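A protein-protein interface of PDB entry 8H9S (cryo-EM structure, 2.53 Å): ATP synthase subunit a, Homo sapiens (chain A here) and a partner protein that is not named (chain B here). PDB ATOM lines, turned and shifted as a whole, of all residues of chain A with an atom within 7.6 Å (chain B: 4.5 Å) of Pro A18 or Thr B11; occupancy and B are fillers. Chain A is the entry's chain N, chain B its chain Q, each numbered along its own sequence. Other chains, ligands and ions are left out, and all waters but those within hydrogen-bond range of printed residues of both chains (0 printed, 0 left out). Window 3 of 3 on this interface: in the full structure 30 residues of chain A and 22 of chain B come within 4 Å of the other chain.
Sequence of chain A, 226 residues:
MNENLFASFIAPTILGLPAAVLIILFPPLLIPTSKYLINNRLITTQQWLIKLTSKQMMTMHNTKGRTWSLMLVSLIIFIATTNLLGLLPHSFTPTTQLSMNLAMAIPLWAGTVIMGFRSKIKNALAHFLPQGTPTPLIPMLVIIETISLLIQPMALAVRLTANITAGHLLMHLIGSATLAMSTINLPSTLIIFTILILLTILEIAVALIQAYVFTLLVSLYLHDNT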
ATOM      1  N   ALA A  11       3.860  -0.851  21.169  1.00  0.00           N
ATOM      2  CA  ALA A  11       3.136   0.393  21.388  1.00  0.00           C
ATOM      3  C   ALA A  11       2.113   0.618  20.285  1.00  0.00           C
ATOM      4  O   ALA A  11       2.487   0.848  19.129  1.00  0.00           O
ATOM      5  CB  ALA A  11       4.105   1.570  21.449  1.00  0.00           C
ATOM      6  N   PRO A  12       0.823   0.558  20.598  1.00  0.00           N
ATOM      7  CA  PRO A  12      -0.192   0.696  19.555  1.00  0.00           C
ATOM      8  C   PRO A  12      -0.237   2.107  19.002  1.00  0.00           C
ATOM      9  O   PRO A  12       0.042   3.084  19.698  1.00  0.00           O
ATOM     10  CB  PRO A  12      -1.488   0.352  20.286  1.00  0.00           C
ATOM     11  CG  PRO A  12      -1.213   0.696  21.688  1.00  0.00           C
ATOM     12  CD  PRO A  12       0.222   0.360  21.923  1.00  0.00           C
ATOM     13  N   THR A  13      -0.595   2.204  17.725  1.00  0.00           N
ATOM     14  CA  THR A  13      -0.755   3.487  17.057  1.00  0.00           C
ATOM     15  C   THR A  13      -1.960   3.408  16.141  1.00  0.00           C
ATOM     16  O   THR A  13      -2.068   2.481  15.336  1.00  0.00           O
ATOM     17  CB  THR A  13       0.486   3.873  16.244  1.00  0.00           C
ATOM     18  OG1 THR A  13       0.854   2.789  15.384  1.00  0.00           O
ATOM     19  CG2 THR A  13       1.653   4.219  17.151  1.00  0.00           C
ATOM     20  N   ILE A  14      -2.858   4.378  16.261  1.00  0.00           N
ATOM     21  CA  ILE A  14      -4.018   4.499  15.386  1.00  0.00           C
ATOM     22  C   ILE A  14      -3.851   5.768  14.563  1.00  0.00           C
ATOM     23  O   ILE A  14      -3.730   6.867  15.117  1.00  0.00           O
ATOM     24  CB  ILE A  14      -5.333   4.496  16.180  1.00  0.00           C
ATOM     25  CG1 ILE A  14      -6.517   4.763  15.255  1.00  0.00           C
ATOM     26  CG2 ILE A  14      -5.284   5.475  17.338  1.00  0.00           C
ATOM     27  CD1 ILE A  14      -6.750   3.673  14.245  1.00  0.00           C
ATOM     28  N   LEU A  15      -3.811   5.608  13.241  1.00  0.00           N
ATOM     29  CA  LEU A  15      -3.614   6.703  12.292  1.00  0.00           C
ATOM     30  C   LEU A  15      -2.346   7.504  12.572  1.00  0.00           C
ATOM     31  O   LEU A  15      -2.246   8.667  12.174  1.00  0.00           O
ATOM     32  CB  LEU A  15      -4.831   7.635  12.261  1.00  0.00           C
ATOM     33  CG  LEU A  15      -6.149   7.000  11.813  1.00  0.00           C
ATOM     34  CD1 LEU A  15      -7.328   7.869  12.207  1.00  0.00           C
ATOM     35  CD2 LEU A  15      -6.149   6.748  10.315  1.00  0.00           C
ATOM     36  N   GLY A  16      -1.370   6.908  13.250  1.00  0.00           N
ATOM     37  CA  GLY A  16      -0.116   7.572  13.533  1.00  0.00           C
ATOM     38  C   GLY A  16       0.000   8.189  14.910  1.00  0.00           C
ATOM     39  O   GLY A  16       1.047   8.766  15.221  1.00  0.00           O
ATOM     40  N   LEU A  17      -1.027   8.084  15.741  1.00  0.00           N
ATOM     41  CA  LEU A  17      -0.982   8.691  17.061  1.00  0.00           C
ATOM     42  C   LEU A  17      -0.768   7.633  18.138  1.00  0.00           C
ATOM     43  O   LEU A  17      -1.153   6.475  17.964  1.00  0.00           O
ATOM     44  CB  LEU A  17      -2.281   9.450  17.342  1.00  0.00           C
ATOM     45  CG  LEU A  17      -2.570  10.632  16.418  1.00  0.00           C
ATOM     46  CD1 LEU A  17      -4.006  11.082  16.572  1.00  0.00           C
ATOM     47  CD2 LEU A  17      -1.622  11.775  16.707  1.00  0.00           C
ATOM     48  N   PRO A  18      -0.169   8.001  19.269  1.00  0.00           N
ATOM     49  CA  PRO A  18       0.084   7.020  20.333  1.00  0.00           C
ATOM     50  C   PRO A  18      -1.156   6.640  21.130  1.00  0.00           C
ATOM     51  O   PRO A  18      -1.433   7.243  22.170  1.00  0.00           O
ATOM     52  CB  PRO A  18       1.114   7.730  21.218  1.00  0.00           C
ATOM     53  CG  PRO A  18       0.869   9.165  20.991  1.00  0.00           C
ATOM     54  CD  PRO A  18       0.471   9.295  19.555  1.00  0.00           C
ATOM     55  N   ALA A  19      -1.917   5.652  20.651  1.00  0.00           N
ATOM     56  CA  ALA A  19      -3.116   5.209  21.357  1.00  0.00           C
ATOM     57  C   ALA A  19      -2.817   4.673  22.751  1.00  0.00           C
ATOM     58  O   ALA A  19      -3.743   4.526  23.560  1.00  0.00           O
ATOM     59  CB  ALA A  19      -3.837   4.141  20.543  1.00  0.00           C
ATOM     60  N   ALA A  20      -1.552   4.374  23.052  1.00  0.00           N
ATOM     61  CA  ALA A  20      -1.200   3.917  24.390  1.00  0.00           C
ATOM     62  C   ALA A  20      -1.579   4.940  25.445  1.00  0.00           C
ATOM     63  O   ALA A  20      -1.896   4.573  26.579  1.00  0.00           O
ATOM     64  CB  ALA A  20       0.292   3.611  24.464  1.00  0.00           C
ATOM     65  N   VAL A  21      -1.582   6.224  25.088  1.00  0.00           N
ATOM     66  CA  VAL A  21      -1.980   7.261  26.034  1.00  0.00           C
ATOM     67  C   VAL A  21      -3.440   7.084  26.430  1.00  0.00           C
ATOM     68  O   VAL A  21      -3.789   7.107  27.616  1.00  0.00           O
ATOM     69  CB  VAL A  21      -1.718   8.653  25.436  1.00  0.00           C
ATOM     70  CG1 VAL A  21      -2.216   9.728  26.368  1.00  0.00           C
ATOM     71  CG2 VAL A  21      -0.239   8.830  25.163  1.00  0.00           C
ATOM     72  N   LEU A  22      -4.317   6.900  25.441  1.00  0.00           N
ATOM     73  CA  LEU A  22      -5.723   6.670  25.743  1.00  0.00           C
ATOM     74  C   LEU A  22      -5.913   5.387  26.534  1.00  0.00           C
ATOM     75  O   LEU A  22      -6.730   5.334  27.460  1.00  0.00           O
ATOM     76  CB  LEU A  22      -6.536   6.620  24.454  1.00  0.00           C
ATOM     77  CG  LEU A  22      -6.588   7.884  23.605  1.00  0.00           C
ATOM     78  CD1 LEU A  22      -7.344   7.613  22.325  1.00  0.00           C
ATOM     79  CD2 LEU A  22      -7.237   9.007  24.377  1.00  0.00           C
ATOM     80  N   ILE A  23      -5.168   4.339  26.186  1.00  0.00           N
ATOM     81  CA  ILE A  23      -5.352   3.064  26.872  1.00  0.00           C
ATOM     82  C   ILE A  23      -4.901   3.154  28.323  1.00  0.00           C
ATOM     83  O   ILE A  23      -5.453   2.473  29.193  1.00  0.00           O
ATOM     84  CB  ILE A  23      -4.618   1.948  26.114  1.00  0.00           C
ATOM     85  CG1 ILE A  23      -5.175   1.825  24.704  1.00  0.00           C
ATOM     86  CG2 ILE A  23      -4.771   0.633  26.819  1.00  0.00           C
ATOM     87  CD1 ILE A  23      -4.413   0.874  23.853  1.00  0.00           C
ATOM     88  N   ILE A  24      -3.905   3.991  28.617  1.00  0.00           N
ATOM     89  CA  ILE A  24      -3.459   4.126  29.999  1.00  0.00           C
ATOM     90  C   ILE A  24      -4.353   5.085  30.776  1.00  0.00           C
ATOM     91  O   ILE A  24      -4.507   4.943  31.992  1.00  0.00           O
ATOM     92  CB  ILE A  24      -1.985   4.562  30.042  1.00  0.00           C
ATOM     93  CG1 ILE A  24      -1.110   3.532  29.341  1.00  0.00           C
ATOM     94  CG2 ILE A  24      -1.512   4.702  31.461  1.00  0.00           C
ATOM     95  CD1 ILE A  24       0.354   3.824  29.428  1.00  0.00           C
ATOM     96  N   SER A  99       8.780  -0.462  31.081  1.00  0.00           N
ATOM     97  CA  SER A  99       8.915   0.962  31.363  1.00  0.00           C
ATOM     98  C   SER A  99       7.891   1.425  32.390  1.00  0.00           C
ATOM     99  O   SER A  99       8.244   2.053  33.394  1.00  0.00           O
ATOM    100  CB  SER A  99       8.764   1.755  30.072  1.00  0.00           C
ATOM    101  OG  SER A  99       7.633   1.317  29.348  1.00  0.00           O
ATOM    102  N   MET A 100       6.612   1.139  32.141  1.00  0.00           N
ATOM    103  CA  MET A 100       5.564   1.546  33.068  1.00  0.00           C
ATOM    104  C   MET A 100       5.756   0.909  34.436  1.00  0.00           C
ATOM    105  O   MET A 100       5.566   1.563  35.466  1.00  0.00           O
ATOM    106  CB  MET A 100       4.198   1.180  32.495  1.00  0.00           C
ATOM    107  CG  MET A 100       3.094   2.131  32.882  1.00  0.00           C
ATOM    108  SD  MET A 100       1.461   1.427  32.655  1.00  0.00           S
ATOM    109  CE  MET A 100       1.379   0.321  34.050  1.00  0.00           C
ATOM    110  N   VAL B   8       9.889   4.227  22.908  1.00  0.00           N
ATOM    111  CA  VAL B   8       8.512   4.476  23.294  1.00  0.00           C
ATOM    112  C   VAL B   8       8.339   4.423  24.812  1.00  0.00           C
ATOM    113  O   VAL B   8       7.229   4.236  25.299  1.00  0.00           O
ATOM    114  CB  VAL B   8       7.549   3.509  22.595  1.00  0.00           C
ATOM    115  CG1 VAL B   8       7.682   3.629  21.096  1.00  0.00           C
ATOM    116  CG2 VAL B   8       7.823   2.091  23.031  1.00  0.00           C
ATOM    117  N   TRP B   9       9.417   4.589  25.566  1.00  0.00           N
ATOM    118  CA  TRP B   9       9.330   4.491  27.015  1.00  0.00           C
ATOM    119  C   TRP B   9       8.659   5.709  27.644  1.00  0.00           C
ATOM    120  O   TRP B   9       7.882   5.539  28.588  1.00  0.00           O
ATOM    121  CB  TRP B   9      10.713   4.272  27.624  1.00  0.00           C
ATOM    122  CG  TRP B   9      11.074   2.829  27.739  1.00  0.00           C
ATOM    123  CD1 TRP B   9      10.638   1.814  26.944  1.00  0.00           C
ATOM    124  CD2 TRP B   9      11.938   2.235  28.710  1.00  0.00           C
ATOM    125  NE1 TRP B   9      11.181   0.626  27.355  1.00  0.00           N
ATOM    126  CE2 TRP B   9      11.985   0.858  28.438  1.00  0.00           C
ATOM    127  CE3 TRP B   9      12.680   2.736  29.781  1.00  0.00           C
ATOM    128  CZ2 TRP B   9      12.739  -0.024  29.198  1.00  0.00           C
ATOM    129  CZ3 TRP B   9      13.428   1.857  30.533  1.00  0.00           C
ATOM    130  CH2 TRP B   9      13.452   0.494  30.240  1.00  0.00           C
ATOM    131  N   PRO B  10       8.919   6.941  27.187  1.00  0.00           N
ATOM    132  CA  PRO B  10       8.156   8.069  27.748  1.00  0.00           C
ATOM    133  C   PRO B  10       6.668   7.991  27.462  1.00  0.00           C
ATOM    134  O   PRO B  10       5.857   8.302  28.341  1.00  0.00           O
ATOM    135  CB  PRO B  10       8.803   9.287  27.082  1.00  0.00           C
ATOM    136  CG  PRO B  10      10.175   8.851  26.796  1.00  0.00           C
ATOM    137  CD  PRO B  10      10.047   7.425  26.375  1.00  0.00           C
ATOM    138  N   THR B  11       6.285   7.563  26.259  1.00  0.00           N
ATOM    139  CA  THR B  11       4.871   7.433  25.929  1.00  0.00           C
ATOM    140  C   THR B  11       4.151   6.504  26.898  1.00  0.00           C
ATOM    141  O   THR B  11       2.949   6.660  27.129  1.00  0.00           O
ATOM    142  CB  THR B  11       4.722   6.938  24.491  1.00  0.00           C
ATOM    143  OG1 THR B  11       5.308   7.891  23.599  1.00  0.00           O
ATOM    144  CG2 THR B  11       3.269   6.759  24.120  1.00  0.00           C
ATOM    145  N   MET B  12       4.863   5.548  27.487  1.00  0.00           N
ATOM    146  CA  MET B  12       4.265   4.645  28.458  1.00  0.00           C
ATOM    147  C   MET B  12       4.379   5.139  29.886  1.00  0.00           C
ATOM    148  O   MET B  12       3.636   4.664  30.748  1.00  0.00           O
ATOM    149  CB  MET B  12       4.914   3.264  28.377  1.00  0.00           C
ATOM    150  CG  MET B  12       4.843   2.625  27.024  1.00  0.00           C
ATOM    151  SD  MET B  12       3.173   2.160  26.593  1.00  0.00           S
ATOM    152  CE  MET B  12       3.416   1.814  24.865  1.00  0.00           C
ATOM    153  N   ILE B  13       5.288   6.065  30.165  1.00  0.00           N
ATOM    154  CA  ILE B  13       5.523   6.525  31.525  1.00  0.00           C
ATOM    155  C   ILE B  13       4.743   7.795  31.829  1.00  0.00           C
ATOM    156  O   ILE B  13       4.244   7.964  32.940  1.00  0.00           O
ATOM    157  CB  ILE B  13       7.033   6.730  31.765  1.00  0.00           C
ATOM    158  CG1 ILE B  13       7.768   5.398  31.699  1.00  0.00           C
ATOM    159  CG2 ILE B  13       7.275   7.367  33.106  1.00  0.00           C
ATOM    160  CD1 ILE B  13       9.253   5.530  31.817  1.00  0.00           C
ATOM    161  N   PRO B  15       1.691   9.169  30.655  1.00  0.00           N
ATOM    162  CA  PRO B  15       0.278   9.055  31.048  1.00  0.00           C
ATOM    163  C   PRO B  15       0.072   8.291  32.340  1.00  0.00           C
ATOM    164  O   PRO B  15      -0.833   8.633  33.109  1.00  0.00           O
ATOM    165  CB  PRO B  15      -0.363   8.341  29.853  1.00  0.00           C
ATOM    166  CG  PRO B  15       0.740   7.728  29.133  1.00  0.00           C
ATOM    167  CD  PRO B  15       1.903   8.623  29.308  1.00  0.00           C
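Printed residues of chain B that touch a printed residue of chain A: Trp B9, Thr B11, Met B12, Ile B13 and Pro B15. Among the printed residues, no Asp or Glu carboxylate lies within 4 Å of a Lys or Arg side-chain nitrogen of the other chain.
Met B12 touches Ala A11 (CE to CB, 3.5 Å). Pro A18 touches Thr B11. Met B12 touches Ala A20. Ile A24 touches Met B12. CD1 of Ile A24 touches CG of Pro B15, at 3.9 Å. Ser A99 touches Trp B9. OG of Ser A99 touches CB of Met B12, 3.5 Å away. O of Ser A99 touches CG1 of Ile B13 (3.8 Å). Met A100 touches Met B12.
Pro A18 touches one residue of chain B. Of the printed residues of chain B, Ala A20 touches Met B12 (3.6 Å). Of the printed residues of chain B, Ile A24 touches Met B12 and Pro B15. Of the printed residues of chain B, Met A100 touches Met B12. Of the printed residues of chain A, Trp B9 touches Ser A99 (3.5 Å). Thr B11 touches one residue of chain A. Printed residues of chain A within 4 Å of Pro B15: Ile A24. The nearest residue of chain A that does not touch Thr B11 is Val A21 (4.2 Å). The nearest printed residue of chain B that does not touch Ala A11 is Val B8 (4.1 Å).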
